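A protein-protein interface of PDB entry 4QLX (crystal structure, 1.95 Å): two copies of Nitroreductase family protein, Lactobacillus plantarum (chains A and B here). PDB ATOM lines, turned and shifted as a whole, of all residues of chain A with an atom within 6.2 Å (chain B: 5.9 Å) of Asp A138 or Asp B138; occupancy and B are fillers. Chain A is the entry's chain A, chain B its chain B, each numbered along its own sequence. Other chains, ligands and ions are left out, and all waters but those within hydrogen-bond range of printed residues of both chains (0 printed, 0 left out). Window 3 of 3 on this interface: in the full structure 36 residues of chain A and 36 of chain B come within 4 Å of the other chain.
Of the 8 printed residues of chain B, 3 touch a printed residue of chain A. Hydrophobic or aromatic side chains of chain B within 4 Å of the printed part of chain A: Phe B142. Hydrophobic or aromatic side chains of chain A within 4 Å of the printed part of chain B: Phe A142. Among the printed residues, 3 pairs touch across the chains. Among the printed residues, no Asp or Glu carboxylate lies within 4 Å of a Lys or Arg side-chain nitrogen of the other chain.
Asp A138 touches its own counterpart, Asp B138. Lys A141 touches Phe B142, and with the chains exchanged Phe A142 touches Lys B141. Positions printed for both chains: 136, 137, 138, 139, 140, 141, 142 and 143. Of the 3 pairs that touch across the chains among the printed residues, 3 have their exchanged pair printed and touching as well.
Lys A141 touches Phe B142. Phe A142 touches Lys B141.
Of the printed residues of chain B, Asp A138 touches Asp B138 (3.4 Å). Printed residues of chain A within 4 Å of Lys B141: Phe A142. Printed residues of chain B within 4 Å of Lys A141: Phe B142 (3.98 Å). Pro A137 touches none of the printed residues of chain B. Phe B139 touches none of the printed residues of chain A. The nearest residue of chain A that does not touch Asp B138 is Lys A141 (6.0 Å). The nearest printed residue of chain B that does not touch Lys A141 is Asp B138 (6.0 Å).
N of Asp A138 sits close to OG1 of Thr A136, at 3.4 Å.
The side-chain carboxylate of Asp B138 sits close to the side-chain carboxylate of Asp A138.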
ATOM      1  N   THR A 136      14.197 -30.903  11.947  1.00  0.00           N
ATOM      2  CA  THR A 136      13.956 -29.917  10.903  1.00  0.00           C
ATOM      3  C   THR A 136      14.437 -28.561  11.391  1.00  0.00           C
ATOM      4  O   THR A 136      14.594 -28.365  12.597  1.00  0.00           O
ATOM      5  CB  THR A 136      12.468 -29.809  10.549  1.00  0.00           C
ATOM      6  OG1 THR A 136      11.803 -29.088  11.591  1.00  0.00           O
ATOM      7  CG2 THR A 136      11.846 -31.187  10.403  1.00  0.00           C
ATOM      8  N   PRO A 137      14.669 -27.617  10.464  1.00  0.00           N
ATOM      9  CA  PRO A 137      15.009 -26.246  10.860  1.00  0.00           C
ATOM     10  C   PRO A 137      13.973 -25.622  11.805  1.00  0.00           C
ATOM     11  O   PRO A 137      14.348 -25.038  12.829  1.00  0.00           O
ATOM     12  CB  PRO A 137      15.056 -25.507   9.520  1.00  0.00           C
ATOM     13  CG  PRO A 137      15.505 -26.563   8.554  1.00  0.00           C
ATOM     14  CD  PRO A 137      14.827 -27.822   9.009  1.00  0.00           C
ATOM     15  N   ASP A 138      12.693 -25.760  11.467  1.00  0.00           N
ATOM     16  CA  ASP A 138      11.606 -25.216  12.287  1.00  0.00           C
ATOM     17  C   ASP A 138      11.739 -25.672  13.746  1.00  0.00           C
ATOM     18  O   ASP A 138      11.634 -24.870  14.666  1.00  0.00           O
ATOM     19  CB  ASP A 138      10.244 -25.629  11.697  1.00  0.00           C
ATOM     20  CG  ASP A 138       9.065 -25.330  12.630  1.00  0.00           C
ATOM     21  OD1 ASP A 138       8.297 -24.384  12.341  1.00  0.00           O
ATOM     22  OD2 ASP A 138       8.878 -26.058  13.635  1.00  0.00           O
ATOM     23  N   PHE A 139      12.013 -26.952  13.953  1.00  0.00           N
ATOM     24  CA  PHE A 139      12.085 -27.477  15.312  1.00  0.00           C
ATOM     25  C   PHE A 139      13.321 -27.023  16.084  1.00  0.00           C
ATOM     26  O   PHE A 139      13.265 -26.866  17.295  1.00  0.00           O
ATOM     27  CB  PHE A 139      12.037 -29.000  15.317  1.00  0.00           C
ATOM     28  CG  PHE A 139      11.831 -29.572  16.687  1.00  0.00           C
ATOM     29  CD1 PHE A 139      10.559 -29.599  17.255  1.00  0.00           C
ATOM     30  CD2 PHE A 139      12.907 -30.041  17.428  1.00  0.00           C
ATOM     31  CE1 PHE A 139      10.361 -30.112  18.529  1.00  0.00           C
ATOM     32  CE2 PHE A 139      12.716 -30.550  18.707  1.00  0.00           C
ATOM     33  CZ  PHE A 139      11.441 -30.585  19.259  1.00  0.00           C
ATOM     34  N   LEU A 140      14.443 -26.847  15.402  1.00  0.00           N
ATOM     35  CA  LEU A 140      15.619 -26.294  16.056  1.00  0.00           C
ATOM     36  C   LEU A 140      15.374 -24.841  16.439  1.00  0.00           C
ATOM     37  O   LEU A 140      15.875 -24.374  17.447  1.00  0.00           O
ATOM     38  CB  LEU A 140      16.853 -26.396  15.150  1.00  0.00           C
ATOM     39  CG  LEU A 140      17.377 -27.798  14.830  1.00  0.00           C
ATOM     40  CD1 LEU A 140      18.534 -27.718  13.844  1.00  0.00           C
ATOM     41  CD2 LEU A 140      17.810 -28.494  16.101  1.00  0.00           C
ATOM     42  N   LYS A 141      14.621 -24.121  15.614  1.00  0.00           N
ATOM     43  CA  LYS A 141      14.313 -22.719  15.888  1.00  0.00           C
ATOM     44  C   LYS A 141      13.368 -22.625  17.091  1.00  0.00           C
ATOM     45  O   LYS A 141      13.530 -21.782  17.967  1.00  0.00           O
ATOM     46  CB  LYS A 141      13.699 -22.057  14.646  1.00  0.00           C
ATOM     47  CG  LYS A 141      13.019 -20.738  14.938  1.00  0.00           C
ATOM     48  CD  LYS A 141      12.322 -20.153  13.716  1.00  0.00           C
ATOM     49  CE  LYS A 141      11.406 -19.001  14.124  1.00  0.00           C
ATOM     50  NZ  LYS A 141      10.846 -18.263  12.951  1.00  0.00           N
ATOM     51  N   PHE A 142      12.393 -23.527  17.125  1.00  0.00           N
ATOM     52  CA  PHE A 142      11.453 -23.664  18.234  1.00  0.00           C
ATOM     53  C   PHE A 142      12.182 -23.963  19.544  1.00  0.00           C
ATOM     54  O   PHE A 142      11.947 -23.310  20.571  1.00  0.00           O
ATOM     55  CB  PHE A 142      10.442 -24.771  17.893  1.00  0.00           C
ATOM     56  CG  PHE A 142       9.595 -25.225  19.052  1.00  0.00           C
ATOM     57  CD1 PHE A 142       8.464 -24.507  19.423  1.00  0.00           C
ATOM     58  CD2 PHE A 142       9.902 -26.389  19.742  1.00  0.00           C
ATOM     59  CE1 PHE A 142       7.671 -24.930  20.481  1.00  0.00           C
ATOM     60  CE2 PHE A 142       9.114 -26.816  20.801  1.00  0.00           C
ATOM     61  CZ  PHE A 142       7.992 -26.083  21.167  1.00  0.00           C
ATOM     62  N   ASP A 143      13.075 -24.949  19.497  1.00  0.00           N
ATOM     63  CA  ASP A 143      13.907 -25.318  20.639  1.00  0.00           C
ATOM     64  C   ASP A 143      14.741 -24.123  21.120  1.00  0.00           C
ATOM     65  O   ASP A 143      14.781 -23.803  22.312  1.00  0.00           O
ATOM     66  CB  ASP A 143      14.819 -26.493  20.257  1.00  0.00           C
ATOM     67  CG  ASP A 143      15.791 -26.886  21.362  1.00  0.00           C
ATOM     68  OD1 ASP A 143      16.897 -26.293  21.456  1.00  0.00           O
ATOM     69  OD2 ASP A 143      15.461 -27.830  22.121  1.00  0.00           O
ATOM     70  N   THR B 136       1.332 -15.654   9.652  1.00  0.00           N
ATOM     71  CA  THR B 136       1.352 -17.055   9.245  1.00  0.00           C
ATOM     72  C   THR B 136       1.034 -17.898  10.467  1.00  0.00           C
ATOM     73  O   THR B 136       1.174 -17.415  11.596  1.00  0.00           O
ATOM     74  CB  THR B 136       2.713 -17.479   8.669  1.00  0.00           C
ATOM     75  OG1 THR B 136       3.720 -17.323   9.672  1.00  0.00           O
ATOM     76  CG2 THR B 136       3.077 -16.642   7.445  1.00  0.00           C
ATOM     77  N   PRO B 137       0.587 -19.152  10.256  1.00  0.00           N
ATOM     78  CA  PRO B 137       0.426 -20.037  11.413  1.00  0.00           C
ATOM     79  C   PRO B 137       1.713 -20.094  12.221  1.00  0.00           C
ATOM     80  O   PRO B 137       1.678 -20.001  13.455  1.00  0.00           O
ATOM     81  CB  PRO B 137       0.107 -21.396  10.780  1.00  0.00           C
ATOM     82  CG  PRO B 137      -0.518 -21.063   9.464  1.00  0.00           C
ATOM     83  CD  PRO B 137       0.157 -19.796   8.999  1.00  0.00           C
ATOM     84  N   ASP B 138       2.836 -20.211  11.516  1.00  0.00           N
ATOM     85  CA  ASP B 138       4.136 -20.355  12.158  1.00  0.00           C
ATOM     86  C   ASP B 138       4.490 -19.156  13.039  1.00  0.00           C
ATOM     87  O   ASP B 138       5.076 -19.327  14.112  1.00  0.00           O
ATOM     88  CB  ASP B 138       5.219 -20.584  11.104  1.00  0.00           C
ATOM     89  CG  ASP B 138       5.388 -22.053  10.760  1.00  0.00           C
ATOM     90  OD1 ASP B 138       4.441 -22.836  11.015  1.00  0.00           O
ATOM     91  OD2 ASP B 138       6.466 -22.429  10.245  1.00  0.00           O
ATOM     92  N   PHE B 139       4.123 -17.951  12.615  1.00  0.00           N
ATOM     93  CA  PHE B 139       4.410 -16.789  13.443  1.00  0.00           C
ATOM     94  C   PHE B 139       3.539 -16.757  14.699  1.00  0.00           C
ATOM     95  O   PHE B 139       3.995 -16.339  15.761  1.00  0.00           O
ATOM     96  CB  PHE B 139       4.236 -15.479  12.674  1.00  0.00           C
ATOM     97  CG  PHE B 139       4.554 -14.276  13.504  1.00  0.00           C
ATOM     98  CD1 PHE B 139       5.869 -14.004  13.866  1.00  0.00           C
ATOM     99  CD2 PHE B 139       3.544 -13.454  13.978  1.00  0.00           C
ATOM    100  CE1 PHE B 139       6.175 -12.914  14.660  1.00  0.00           C
ATOM    101  CE2 PHE B 139       3.840 -12.356  14.771  1.00  0.00           C
ATOM    102  CZ  PHE B 139       5.159 -12.094  15.113  1.00  0.00           C
ATOM    103  N   LEU B 140       2.286 -17.181  14.589  1.00  0.00           N
ATOM    104  CA  LEU B 140       1.439 -17.267  15.779  1.00  0.00           C
ATOM    105  C   LEU B 140       1.969 -18.347  16.737  1.00  0.00           C
ATOM    106  O   LEU B 140       1.923 -18.193  17.959  1.00  0.00           O
ATOM    107  CB  LEU B 140      -0.013 -17.561  15.398  1.00  0.00           C
ATOM    108  CG  LEU B 140      -0.787 -16.446  14.679  1.00  0.00           C
ATOM    109  CD1 LEU B 140      -2.252 -16.838  14.502  1.00  0.00           C
ATOM    110  CD2 LEU B 140      -0.667 -15.129  15.418  1.00  0.00           C
ATOM    111  N   LYS B 141       2.470 -19.436  16.173  1.00  0.00           N
ATOM    112  CA  LYS B 141       3.050 -20.516  16.971  1.00  0.00           C
ATOM    113  C   LYS B 141       4.277 -20.036  17.751  1.00  0.00           C
ATOM    114  O   LYS B 141       4.411 -20.272  18.954  1.00  0.00           O
ATOM    115  CB  LYS B 141       3.415 -21.698  16.069  1.00  0.00           C
ATOM    116  CG  LYS B 141       4.227 -22.778  16.746  1.00  0.00           C
ATOM    117  CD  LYS B 141       4.445 -23.946  15.808  1.00  0.00           C
ATOM    118  CE  LYS B 141       5.347 -24.992  16.434  1.00  0.00           C
ATOM    119  NZ  LYS B 141       6.722 -24.454  16.631  1.00  0.00           N
ATOM    120  N   PHE B 142       5.172 -19.356  17.043  1.00  0.00           N
ATOM    121  CA  PHE B 142       6.365 -18.764  17.631  1.00  0.00           C
ATOM    122  C   PHE B 142       5.983 -17.776  18.753  1.00  0.00           C
ATOM    123  O   PHE B 142       6.513 -17.854  19.869  1.00  0.00           O
ATOM    124  CB  PHE B 142       7.174 -18.114  16.489  1.00  0.00           C
ATOM    125  CG  PHE B 142       8.176 -17.080  16.919  1.00  0.00           C
ATOM    126  CD1 PHE B 142       9.479 -17.442  17.239  1.00  0.00           C
ATOM    127  CD2 PHE B 142       7.838 -15.737  16.925  1.00  0.00           C
ATOM    128  CE1 PHE B 142      10.419 -16.481  17.605  1.00  0.00           C
ATOM    129  CE2 PHE B 142       8.768 -14.771  17.290  1.00  0.00           C
ATOM    130  CZ  PHE B 142      10.063 -15.147  17.630  1.00  0.00           C
ATOM    131  N   ASP B 143       5.028 -16.888  18.470  1.00  0.00           N
ATOM    132  CA  ASP B 143       4.559 -15.894  19.446  1.00  0.00           C
ATOM    133  C   ASP B 143       4.059 -16.527  20.746  1.00  0.00           C
ATOM    134  O   ASP B 143       4.440 -16.102  21.839  1.00  0.00           O
ATOM    135  CB  ASP B 143       3.444 -15.035  18.828  1.00  0.00           C
ATOM    136  CG  ASP B 143       2.871 -14.002  19.802  1.00  0.00           C
ATOM    137  OD1 ASP B 143       3.347 -12.849  19.796  1.00  0.00           O
ATOM    138  OD2 ASP B 143       1.935 -14.334  20.565  1.00  0.00           O
